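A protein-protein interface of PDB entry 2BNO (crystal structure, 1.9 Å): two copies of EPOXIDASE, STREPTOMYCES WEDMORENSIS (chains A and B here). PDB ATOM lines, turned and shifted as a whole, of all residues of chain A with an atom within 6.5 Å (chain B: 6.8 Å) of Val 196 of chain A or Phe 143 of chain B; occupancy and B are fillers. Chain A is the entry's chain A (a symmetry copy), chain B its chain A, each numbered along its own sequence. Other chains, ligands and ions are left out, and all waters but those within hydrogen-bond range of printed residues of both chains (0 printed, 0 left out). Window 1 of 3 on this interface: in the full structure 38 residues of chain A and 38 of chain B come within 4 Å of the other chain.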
ATOM      1  N   LEU A 108      -8.436 -10.319   5.497  1.00  0.00           N
ATOM      2  CA  LEU A 108      -9.014 -11.455   4.813  1.00  0.00           C
ATOM      3  C   LEU A 108      -9.266 -12.632   5.783  1.00  0.00           C
ATOM      4  O   LEU A 108      -9.097 -12.473   7.006  1.00  0.00           O
ATOM      5  CB  LEU A 108      -8.125 -11.902   3.613  1.00  0.00           C
ATOM      6  CG  LEU A 108      -7.797 -10.689   2.715  1.00  0.00           C
ATOM      7  CD1 LEU A 108      -6.759 -11.098   1.648  1.00  0.00           C
ATOM      8  CD2 LEU A 108      -9.077 -10.206   2.026  1.00  0.00           C
ATOM      9  N   VAL A 109      -9.734 -13.744   5.238  1.00  0.00           N
ATOM     10  CA  VAL A 109     -10.162 -14.928   5.997  1.00  0.00           C
ATOM     11  C   VAL A 109      -9.061 -15.376   6.979  1.00  0.00           C
ATOM     12  O   VAL A 109      -7.853 -15.387   6.649  1.00  0.00           O
ATOM     13  CB  VAL A 109     -10.605 -16.106   5.058  1.00  0.00           C
ATOM     14  CG1 VAL A 109      -9.403 -16.775   4.305  1.00  0.00           C
ATOM     15  CG2 VAL A 109     -11.438 -17.148   5.779  1.00  0.00           C
ATOM     16  N   LEU A 117      -1.823 -17.670  10.384  1.00  0.00           N
ATOM     17  CA  LEU A 117      -2.193 -17.182   9.043  1.00  0.00           C
ATOM     18  C   LEU A 117      -2.980 -15.896   9.142  1.00  0.00           C
ATOM     19  O   LEU A 117      -4.150 -15.897   9.594  1.00  0.00           O
ATOM     20  CB  LEU A 117      -3.036 -18.231   8.286  1.00  0.00           C
ATOM     21  CG  LEU A 117      -3.552 -17.799   6.906  1.00  0.00           C
ATOM     22  CD1 LEU A 117      -2.402 -17.658   5.869  1.00  0.00           C
ATOM     23  CD2 LEU A 117      -4.642 -18.789   6.396  1.00  0.00           C
ATOM     24  N   VAL A 118      -2.369 -14.798   8.709  1.00  0.00           N
ATOM     25  CA  VAL A 118      -3.061 -13.494   8.742  1.00  0.00           C
ATOM     26  C   VAL A 118      -2.926 -12.844   7.358  1.00  0.00           C
ATOM     27  O   VAL A 118      -1.912 -12.209   7.094  1.00  0.00           O
ATOM     28  CB  VAL A 118      -2.529 -12.537   9.848  1.00  0.00           C
ATOM     29  CG1 VAL A 118      -3.424 -11.178   9.877  1.00  0.00           C
ATOM     30  CG2 VAL A 118      -2.544 -13.231  11.272  1.00  0.00           C
ATOM     31  N   PRO A 119      -3.879 -13.062   6.452  1.00  0.00           N
ATOM     32  CA  PRO A 119      -3.821 -12.422   5.149  1.00  0.00           C
ATOM     33  C   PRO A 119      -4.575 -11.083   5.126  1.00  0.00           C
ATOM     34  O   PRO A 119      -5.680 -10.955   5.702  1.00  0.00           O
ATOM     35  CB  PRO A 119      -4.463 -13.438   4.210  1.00  0.00           C
ATOM     36  CG  PRO A 119      -5.267 -14.434   5.148  1.00  0.00           C
ATOM     37  CD  PRO A 119      -4.977 -14.035   6.554  1.00  0.00           C
ATOM     38  N   LEU A 120      -3.983 -10.096   4.455  1.00  0.00           N
ATOM     39  CA  LEU A 120      -4.549  -8.741   4.416  1.00  0.00           C
ATOM     40  C   LEU A 120      -4.551  -8.255   2.985  1.00  0.00           C
ATOM     41  O   LEU A 120      -3.692  -8.644   2.193  1.00  0.00           O
ATOM     42  CB  LEU A 120      -3.666  -7.768   5.211  1.00  0.00           C
ATOM     43  CG  LEU A 120      -3.326  -8.123   6.655  1.00  0.00           C
ATOM     44  CD1 LEU A 120      -2.203  -7.224   7.201  1.00  0.00           C
ATOM     45  CD2 LEU A 120      -4.612  -8.075   7.518  1.00  0.00           C
ATOM     46  N   ASN A 141       7.108 -15.991   8.475  1.00  0.00           N
ATOM     47  CA  ASN A 141       7.389 -15.555   7.102  1.00  0.00           C
ATOM     48  C   ASN A 141       6.209 -14.789   6.509  1.00  0.00           C
ATOM     49  O   ASN A 141       5.083 -14.828   7.053  1.00  0.00           O
ATOM     50  CB  ASN A 141       7.739 -16.761   6.229  1.00  0.00           C
ATOM     51  CG  ASN A 141       8.990 -17.482   6.709  1.00  0.00           C
ATOM     52  OD1 ASN A 141       9.895 -16.862   7.254  1.00  0.00           O
ATOM     53  ND2 ASN A 141       9.025 -18.797   6.535  1.00  0.00           N
ATOM     54  N   GLU A 142       6.456 -14.102   5.396  1.00  0.00           N
ATOM     55  CA  GLU A 142       5.392 -13.365   4.713  1.00  0.00           C
ATOM     56  C   GLU A 142       5.516 -13.527   3.229  1.00  0.00           C
ATOM     57  O   GLU A 142       6.629 -13.451   2.711  1.00  0.00           O
ATOM     58  CB  GLU A 142       5.459 -11.872   5.082  1.00  0.00           C
ATOM     59  CG  GLU A 142       4.302 -11.044   4.509  1.00  0.00           C
ATOM     60  CD  GLU A 142       4.295  -9.620   5.067  1.00  0.00           C
ATOM     61  OE1 GLU A 142       5.328  -9.184   5.628  1.00  0.00           O
ATOM     62  OE2 GLU A 142       3.264  -8.936   4.965  1.00  0.00           O
ATOM     63  N   PHE A 143       4.373 -13.747   2.547  1.00  0.00           N
ATOM     64  CA  PHE A 143       4.302 -13.770   1.095  1.00  0.00           C
ATOM     65  C   PHE A 143       3.514 -12.515   0.661  1.00  0.00           C
ATOM     66  O   PHE A 143       2.486 -12.212   1.281  1.00  0.00           O
ATOM     67  CB  PHE A 143       3.544 -15.018   0.625  1.00  0.00           C
ATOM     68  CG  PHE A 143       3.054 -14.913  -0.815  1.00  0.00           C
ATOM     69  CD1 PHE A 143       3.952 -15.086  -1.887  1.00  0.00           C
ATOM     70  CD2 PHE A 143       1.726 -14.575  -1.102  1.00  0.00           C
ATOM     71  CE1 PHE A 143       3.523 -14.924  -3.207  1.00  0.00           C
ATOM     72  CE2 PHE A 143       1.283 -14.425  -2.417  1.00  0.00           C
ATOM     73  CZ  PHE A 143       2.177 -14.603  -3.478  1.00  0.00           C
ATOM     74  N   LEU A 144       3.991 -11.792  -0.369  1.00  0.00           N
ATOM     75  CA  LEU A 144       3.289 -10.554  -0.847  1.00  0.00           C
ATOM     76  C   LEU A 144       3.065 -10.623  -2.359  1.00  0.00           C
ATOM     77  O   LEU A 144       3.881 -11.220  -3.077  1.00  0.00           O
ATOM     78  CB  LEU A 144       4.074  -9.292  -0.477  1.00  0.00           C
ATOM     79  CG  LEU A 144       4.204  -9.022   1.034  1.00  0.00           C
ATOM     80  CD1 LEU A 144       5.604  -9.469   1.500  1.00  0.00           C
ATOM     81  CD2 LEU A 144       3.878  -7.548   1.447  1.00  0.00           C
ATOM     82  N   PHE A 145       1.976 -10.014  -2.836  1.00  0.00           N
ATOM     83  CA  PHE A 145       1.652  -9.983  -4.263  1.00  0.00           C
ATOM     84  C   PHE A 145       1.114  -8.559  -4.546  1.00  0.00           C
ATOM     85  O   PHE A 145       0.235  -8.070  -3.839  1.00  0.00           O
ATOM     86  CB  PHE A 145       0.577 -11.016  -4.588  1.00  0.00           C
ATOM     87  CG  PHE A 145       0.131 -11.036  -6.036  1.00  0.00           C
ATOM     88  CD1 PHE A 145       0.875 -11.702  -7.007  1.00  0.00           C
ATOM     89  CD2 PHE A 145      -1.046 -10.371  -6.431  1.00  0.00           C
ATOM     90  CE1 PHE A 145       0.447 -11.755  -8.345  1.00  0.00           C
ATOM     91  CE2 PHE A 145      -1.466 -10.379  -7.794  1.00  0.00           C
ATOM     92  CZ  PHE A 145      -0.724 -11.096  -8.742  1.00  0.00           C
ATOM     93  N   ILE A 194      -1.469  -7.714  -1.605  1.00  0.00           N
ATOM     94  CA  ILE A 194      -1.993  -8.730  -0.668  1.00  0.00           C
ATOM     95  C   ILE A 194      -0.784  -9.210   0.106  1.00  0.00           C
ATOM     96  O   ILE A 194       0.244  -9.555  -0.503  1.00  0.00           O
ATOM     97  CB  ILE A 194      -2.560  -9.975  -1.357  1.00  0.00           C
ATOM     98  CG1 ILE A 194      -3.746  -9.643  -2.232  1.00  0.00           C
ATOM     99  CG2 ILE A 194      -2.944 -11.060  -0.279  1.00  0.00           C
ATOM    100  CD1 ILE A 194      -4.102 -10.787  -3.174  1.00  0.00           C
ATOM    101  N   ALA A 195      -0.891  -9.153   1.429  1.00  0.00           N
ATOM    102  CA  ALA A 195       0.135  -9.634   2.308  1.00  0.00           C
ATOM    103  C   ALA A 195      -0.384 -10.867   3.062  1.00  0.00           C
ATOM    104  O   ALA A 195      -1.412 -10.801   3.746  1.00  0.00           O
ATOM    105  CB  ALA A 195       0.504  -8.573   3.292  1.00  0.00           C
ATOM    106  N   VAL A 196       0.359 -11.959   2.980  1.00  0.00           N
ATOM    107  CA  VAL A 196      -0.033 -13.167   3.677  1.00  0.00           C
ATOM    108  C   VAL A 196       1.058 -13.507   4.688  1.00  0.00           C
ATOM    109  O   VAL A 196       2.118 -14.027   4.343  1.00  0.00           O
ATOM    110  CB  VAL A 196      -0.257 -14.325   2.698  1.00  0.00           C
ATOM    111  CG1 VAL A 196      -0.720 -15.612   3.463  1.00  0.00           C
ATOM    112  CG2 VAL A 196      -1.237 -13.921   1.515  1.00  0.00           C
ATOM    113  N   ASN A 197       0.805 -13.200   5.954  1.00  0.00           N
ATOM    114  CA  ASN A 197       1.710 -13.651   7.010  1.00  0.00           C
ATOM    115  C   ASN A 197       1.294 -15.079   7.355  1.00  0.00           C
ATOM    116  O   ASN A 197       0.109 -15.385   7.375  1.00  0.00           O
ATOM    117  CB  ASN A 197       1.641 -12.709   8.214  1.00  0.00           C
ATOM    118  CG  ASN A 197       2.476 -11.458   7.998  1.00  0.00           C
ATOM    119  OD1 ASN A 197       1.983 -10.437   7.540  1.00  0.00           O
ATOM    120  ND2 ASN A 197       3.754 -11.552   8.290  1.00  0.00           N
ATOM    121  N   PHE A 198       2.241 -15.986   7.545  1.00  0.00           N
ATOM    122  CA  PHE A 198       1.836 -17.395   7.773  1.00  0.00           C
ATOM    123  C   PHE A 198       2.751 -18.077   8.764  1.00  0.00           C
ATOM    124  O   PHE A 198       3.710 -17.480   9.246  1.00  0.00           O
ATOM    125  CB  PHE A 198       1.690 -18.223   6.459  1.00  0.00           C
ATOM    126  CG  PHE A 198       2.955 -18.331   5.647  1.00  0.00           C
ATOM    127  CD1 PHE A 198       3.773 -19.471   5.736  1.00  0.00           C
ATOM    128  CD2 PHE A 198       3.337 -17.298   4.776  1.00  0.00           C
ATOM    129  CE1 PHE A 198       4.948 -19.567   4.970  1.00  0.00           C
ATOM    130  CE2 PHE A 198       4.479 -17.372   4.023  1.00  0.00           C
ATOM    131  CZ  PHE A 198       5.297 -18.505   4.099  1.00  0.00           C
ATOM    132  OXT PHE A 198       2.491 -19.242   9.105  1.00  0.00           O
ATOM    133  N   ASN B 141      -1.771 -26.755   4.133  1.00  0.00           N
ATOM    134  CA  ASN B 141      -2.930 -25.864   4.012  1.00  0.00           C
ATOM    135  C   ASN B 141      -2.834 -24.992   2.762  1.00  0.00           C
ATOM    136  O   ASN B 141      -1.754 -24.884   2.140  1.00  0.00           O
ATOM    137  CB  ASN B 141      -3.058 -24.994   5.263  1.00  0.00           C
ATOM    138  CG  ASN B 141      -3.287 -25.817   6.522  1.00  0.00           C
ATOM    139  OD1 ASN B 141      -3.901 -26.875   6.471  1.00  0.00           O
ATOM    140  ND2 ASN B 141      -2.762 -25.347   7.647  1.00  0.00           N
ATOM    141  N   GLU B 142      -3.950 -24.366   2.396  1.00  0.00           N
ATOM    142  CA  GLU B 142      -3.967 -23.469   1.240  1.00  0.00           C
ATOM    143  C   GLU B 142      -4.789 -22.252   1.537  1.00  0.00           C
ATOM    144  O   GLU B 142      -5.864 -22.386   2.119  1.00  0.00           O
ATOM    145  CB  GLU B 142      -4.540 -24.198   0.011  1.00  0.00           C
ATOM    146  CG  GLU B 142      -4.478 -23.371  -1.279  1.00  0.00           C
ATOM    147  CD  GLU B 142      -4.863 -24.203  -2.504  1.00  0.00           C
ATOM    148  OE1 GLU B 142      -5.466 -25.290  -2.333  1.00  0.00           O
ATOM    149  OE2 GLU B 142      -4.557 -23.792  -3.633  1.00  0.00           O
ATOM    150  N   PHE B 143      -4.285 -21.069   1.133  1.00  0.00           N
ATOM    151  CA  PHE B 143      -5.025 -19.819   1.205  1.00  0.00           C
ATOM    152  C   PHE B 143      -5.345 -19.399  -0.247  1.00  0.00           C
ATOM    153  O   PHE B 143      -4.457 -19.492  -1.104  1.00  0.00           O
ATOM    154  CB  PHE B 143      -4.160 -18.732   1.856  1.00  0.00           C
ATOM    155  CG  PHE B 143      -4.674 -17.321   1.589  1.00  0.00           C
ATOM    156  CD1 PHE B 143      -5.787 -16.823   2.295  1.00  0.00           C
ATOM    157  CD2 PHE B 143      -4.099 -16.520   0.595  1.00  0.00           C
ATOM    158  CE1 PHE B 143      -6.303 -15.557   2.007  1.00  0.00           C
ATOM    159  CE2 PHE B 143      -4.597 -15.248   0.308  1.00  0.00           C
ATOM    160  CZ  PHE B 143      -5.699 -14.756   1.016  1.00  0.00           C
ATOM    161  N   LEU B 144      -6.589 -18.965  -0.520  1.00  0.00           N
ATOM    162  CA  LEU B 144      -6.983 -18.545  -1.908  1.00  0.00           C
ATOM    163  C   LEU B 144      -7.630 -17.160  -1.877  1.00  0.00           C
ATOM    164  O   LEU B 144      -8.286 -16.805  -0.886  1.00  0.00           O
ATOM    165  CB  LEU B 144      -7.928 -19.567  -2.548  1.00  0.00           C
ATOM    166  CG  LEU B 144      -7.315 -20.958  -2.797  1.00  0.00           C
ATOM    167  CD1 LEU B 144      -7.786 -21.915  -1.683  1.00  0.00           C
ATOM    168  CD2 LEU B 144      -7.589 -21.526  -4.229  1.00  0.00           C
ATOM    169  N   PHE B 145      -7.455 -16.389  -2.955  1.00  0.00           N
ATOM    170  CA  PHE B 145      -8.037 -15.051  -3.068  1.00  0.00           C
ATOM    171  C   PHE B 145      -8.526 -14.923  -4.532  1.00  0.00           C
ATOM    172  O   PHE B 145      -7.781 -15.209  -5.468  1.00  0.00           O
ATOM    173  CB  PHE B 145      -6.984 -13.985  -2.780  1.00  0.00           C
ATOM    174  CG  PHE B 145      -7.470 -12.556  -2.918  1.00  0.00           C
ATOM    175  CD1 PHE B 145      -8.182 -11.939  -1.893  1.00  0.00           C
ATOM    176  CD2 PHE B 145      -7.217 -11.825  -4.095  1.00  0.00           C
ATOM    177  CE1 PHE B 145      -8.604 -10.602  -2.000  1.00  0.00           C
ATOM    178  CE2 PHE B 145      -7.680 -10.483  -4.233  1.00  0.00           C
ATOM    179  CZ  PHE B 145      -8.353  -9.871  -3.168  1.00  0.00           C
ATOM    180  N   ALA B 170     -13.230 -12.367  -2.770  1.00  0.00           N
ATOM    181  CA  ALA B 170     -13.497 -13.385  -1.740  1.00  0.00           C
ATOM    182  C   ALA B 170     -12.168 -14.069  -1.338  1.00  0.00           C
ATOM    183  O   ALA B 170     -11.232 -14.171  -2.160  1.00  0.00           O
ATOM    184  CB  ALA B 170     -14.514 -14.432  -2.236  1.00  0.00           C
ATOM    185  N   SER B 171     -12.084 -14.544  -0.100  1.00  0.00           N
ATOM    186  CA  SER B 171     -10.892 -15.317   0.287  1.00  0.00           C
ATOM    187  C   SER B 171     -11.310 -16.635   0.953  1.00  0.00           C
ATOM    188  O   SER B 171     -12.440 -16.756   1.453  1.00  0.00           O
ATOM    189  CB  SER B 171      -9.955 -14.487   1.148  1.00  0.00           C
ATOM    190  OG  SER B 171     -10.624 -14.063   2.323  1.00  0.00           O
ATOM    191  N   MET B 172     -10.425 -17.623   0.914  1.00  0.00           N
ATOM    192  CA  MET B 172     -10.769 -18.951   1.370  1.00  0.00           C
ATOM    193  C   MET B 172      -9.558 -19.633   1.981  1.00  0.00           C
ATOM    194  O   MET B 172      -8.414 -19.363   1.591  1.00  0.00           O
ATOM    195  CB  MET B 172     -11.313 -19.761   0.213  1.00  0.00           C
ATOM    196  CG  MET B 172     -11.655 -21.163   0.558  1.00  0.00           C
ATOM    197  SD  MET B 172     -12.594 -21.856  -0.801  1.00  0.00           S
ATOM    198  CE  MET B 172     -12.048 -23.545  -0.764  1.00  0.00           C
ATOM    199  N   PHE B 173      -9.826 -20.522   2.932  1.00  0.00           N
ATOM    200  CA  PHE B 173      -8.807 -21.384   3.497  1.00  0.00           C
ATOM    201  C   PHE B 173      -9.249 -22.817   3.312  1.00  0.00           C
ATOM    202  O   PHE B 173     -10.416 -23.169   3.601  1.00  0.00           O
ATOM    203  CB  PHE B 173      -8.634 -21.057   4.993  1.00  0.00           C
ATOM    204  CG  PHE B 173      -7.778 -22.082   5.740  1.00  0.00           C
ATOM    205  CD1 PHE B 173      -6.390 -21.894   5.862  1.00  0.00           C
ATOM    206  CD2 PHE B 173      -8.373 -23.194   6.346  1.00  0.00           C
ATOM    207  CE1 PHE B 173      -5.582 -22.821   6.580  1.00  0.00           C
ATOM    208  CE2 PHE B 173      -7.574 -24.146   7.049  1.00  0.00           C
ATOM    209  CZ  PHE B 173      -6.175 -23.953   7.140  1.00  0.00           C
ATOM    210  N   VAL B 174      -8.334 -23.652   2.825  1.00  0.00           N
ATOM    211  CA  VAL B 174      -8.612 -25.074   2.634  1.00  0.00           C
ATOM    212  C   VAL B 174      -7.596 -25.843   3.480  1.00  0.00           C
ATOM    213  O   VAL B 174      -6.352 -25.699   3.287  1.00  0.00           O
ATOM    214  CB  VAL B 174      -8.465 -25.517   1.130  1.00  0.00           C
ATOM    215  CG1 VAL B 174      -8.801 -27.001   0.976  1.00  0.00           C
ATOM    216  CG2 VAL B 174      -9.381 -24.709   0.248  1.00  0.00           C
ATOM    217  N   LEU B 193      -7.631 -16.800  -9.777  1.00  0.00           N
ATOM    218  CA  LEU B 193      -7.402 -16.685  -8.353  1.00  0.00           C
ATOM    219  C   LEU B 193      -5.926 -16.768  -8.040  1.00  0.00           C
ATOM    220  O   LEU B 193      -5.102 -17.199  -8.911  1.00  0.00           O
ATOM    221  CB  LEU B 193      -8.205 -17.745  -7.635  1.00  0.00           C
ATOM    222  CG  LEU B 193      -7.955 -19.165  -8.056  1.00  0.00           C
ATOM    223  CD1 LEU B 193      -6.786 -19.696  -7.289  1.00  0.00           C
ATOM    224  CD2 LEU B 193      -9.181 -19.953  -7.753  1.00  0.00           C
ATOM    225  N   ILE B 194      -5.573 -16.328  -6.843  1.00  0.00           N
ATOM    226  CA  ILE B 194      -4.205 -16.586  -6.346  1.00  0.00           C
ATOM    227  C   ILE B 194      -4.361 -17.696  -5.329  1.00  0.00           C
ATOM    228  O   ILE B 194      -5.223 -17.603  -4.437  1.00  0.00           O
ATOM    229  CB  ILE B 194      -3.592 -15.410  -5.578  1.00  0.00           C
ATOM    230  CG1 ILE B 194      -3.435 -14.189  -6.453  1.00  0.00           C
ATOM    231  CG2 ILE B 194      -2.208 -15.837  -4.955  1.00  0.00           C
ATOM    232  CD1 ILE B 194      -3.154 -12.932  -5.638  1.00  0.00           C
ATOM    233  N   ALA B 195      -3.588 -18.760  -5.519  1.00  0.00           N
ATOM    234  CA  ALA B 195      -3.563 -19.869  -4.609  1.00  0.00           C
ATOM    235  C   ALA B 195      -2.193 -19.921  -3.916  1.00  0.00           C
ATOM    236  O   ALA B 195      -1.154 -20.004  -4.580  1.00  0.00           O
ATOM    237  CB  ALA B 195      -3.789 -21.144  -5.351  1.00  0.00           C
ATOM    238  N   VAL B 196      -2.206 -19.930  -2.593  1.00  0.00           N
ATOM    239  CA  VAL B 196      -0.966 -20.004  -1.847  1.00  0.00           C
ATOM    240  C   VAL B 196      -0.981 -21.291  -1.027  1.00  0.00           C
ATOM    241  O   VAL B 196      -1.633 -21.386   0.011  1.00  0.00           O
ATOM    242  CB  VAL B 196      -0.788 -18.779  -0.946  1.00  0.00           C
ATOM    243  CG1 VAL B 196       0.576 -18.852  -0.178  1.00  0.00           C
ATOM    244  CG2 VAL B 196      -0.974 -17.419  -1.747  1.00  0.00           C
ATOM    245  N   ASN B 197      -0.263 -22.301  -1.502  1.00  0.00           N
ATOM    246  CA  ASN B 197      -0.073 -23.505  -0.695  1.00  0.00           C
ATOM    247  C   ASN B 197       1.098 -23.216   0.243  1.00  0.00           C
ATOM    248  O   ASN B 197       2.060 -22.573  -0.157  1.00  0.00           O
ATOM    249  CB  ASN B 197       0.176 -24.719  -1.593  1.00  0.00           C
ATOM    250  CG  ASN B 197      -1.119 -25.274  -2.161  1.00  0.00           C
ATOM    251  OD1 ASN B 197      -1.538 -24.917  -3.253  1.00  0.00           O
ATOM    252  ND2 ASN B 197      -1.777 -26.117  -1.397  1.00  0.00           N
ATOM    253  N   PHE B 198       1.006 -23.601   1.507  1.00  0.00           N
ATOM    254  CA  PHE B 198       2.094 -23.225   2.442  1.00  0.00           C
ATOM    255  C   PHE B 198       2.355 -24.320   3.451  1.00  0.00           C
ATOM    256  O   PHE B 198       1.681 -25.346   3.452  1.00  0.00           O
ATOM    257  CB  PHE B 198       1.875 -21.844   3.134  1.00  0.00           C
ATOM    258  CG  PHE B 198       0.625 -21.759   3.971  1.00  0.00           C
ATOM    259  CD1 PHE B 198       0.679 -21.936   5.365  1.00  0.00           C
ATOM    260  CD2 PHE B 198      -0.619 -21.490   3.378  1.00  0.00           C
ATOM    261  CE1 PHE B 198      -0.492 -21.849   6.141  1.00  0.00           C
ATOM    262  CE2 PHE B 198      -1.769 -21.403   4.116  1.00  0.00           C
ATOM    263  CZ  PHE B 198      -1.726 -21.571   5.504  1.00  0.00           C
ATOM    264  OXT PHE B 198       3.289 -24.172   4.256  1.00  0.00           O
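Printed residues of chain B that touch a printed residue of chain A: Phe 143, Phe 145, Ser 171, Met 172, Phe 173, Ile 194, Val 196 and Phe 198. Of the 16 printed residues of chain A, 9 touch a printed residue of chain B. Hydrophobic or aromatic side chains of chain A that line the printed part of chain B: Leu 108, Val 109, Leu 117, Pro 119, Phe 143, Phe 145, Ile 194, Val 196 and Phe 198. Among the printed residues, 14 pairs touch across the chains. Among the printed residues, no Asp or Glu carboxylate lies within 4 Å of a Lys or Arg side-chain nitrogen of the other chain.
Val 196 of chain A touches just one residue of chain B: Phe 143 (3.8 Å). Of the printed residues of chain A, Phe 173 of chain B touches Leu 117 (3.6 Å). Of the printed residues of chain B, Phe 198 of chain A touches Phe 198. Val 118 of chain A touches none of the printed residues of chain B. Ala 195 of chain A touches none of the printed residues of chain B. The nearest printed residue of chain A that does not touch Met 172 of chain B is Leu 117 of chain A (6.1 Å).
N of Val 109 of chain A lies within hydrogen-bond range of OG of Ser 171 of chain B (3.1 Å).
Phe 143 of chain A touches Val 196 of chain B, and with the chains exchanged Val 196 of chain A touches Phe 143 of chain B. Phe 145 of chain A touches Ile 194 of chain B, and with the chains exchanged Ile 194 of chain A touches Phe 145 of chain B. Ile 194 of chain B touches its own counterpart, Ile 194 of chain A. Phe 198 of chain A touches its own counterpart, Phe 198 of chain B. Of the 14 pairs that touch across the chains among the printed residues, 6 have their exchanged pair printed and touching as well.
CD1 of Leu 108 of chain A touches CZ of Phe 143 of chain B, at 3.9 Å. CD1 of Phe 145 of chain B touches CD1 of Leu 108 of chain A, 3.9 Å away. N of Met 172 of chain B touches CG1 of Val 109 of chain A, 3.6 Å away. Leu 117 of chain A touches Phe 173 of chain B. CD1 of Leu 117 of chain A touches CZ of Phe 198 of chain B, at 3.99 Å. Phe 143 of chain A touches Val 196 of chain B (CE2 to CG2, 3.8 Å). Phe 145 of chain A touches Ile 194 of chain B (CD2 to CD1, 3.4 Å). CD1 of Ile 194 of chain A touches CD2 of Phe 145 of chain B (3.4 Å). Phe 143 of chain B touches Val 196 of chain A (CE2 to CG2, 3.8 Å). Phe 198 of chain B touches Phe 198 of chain A.
The backbone NH (N) of Ile 194 of chain A lies within hydrogen-bond range of the backbone carbonyl oxygen (O) of Phe 145 of chain A, at 2.8 Å. N of Phe 198 of chain A sits at hydrogen-bond distance from O of Asn 141 of chain A, at 3.1 Å. The backbone NH (N) of Leu 144 of chain B lies within hydrogen-bond range of the backbone carbonyl oxygen (O) of Met 172 of chain B (2.8 Å). The backbone NH (N) of Phe 198 of chain B sits at hydrogen-bond distance from the backbone carbonyl oxygen (O) of Asn 141 of chain B (3.1 Å). The backbone NH of Val 196 of chain B is in hydrogen-bond range of the backbone carbonyl oxygen of Phe 143 of chain B, 2.7 Å away. O of Phe 145 of chain B lies within hydrogen-bond range of N of Ile 194 of chain B (2.8 Å).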
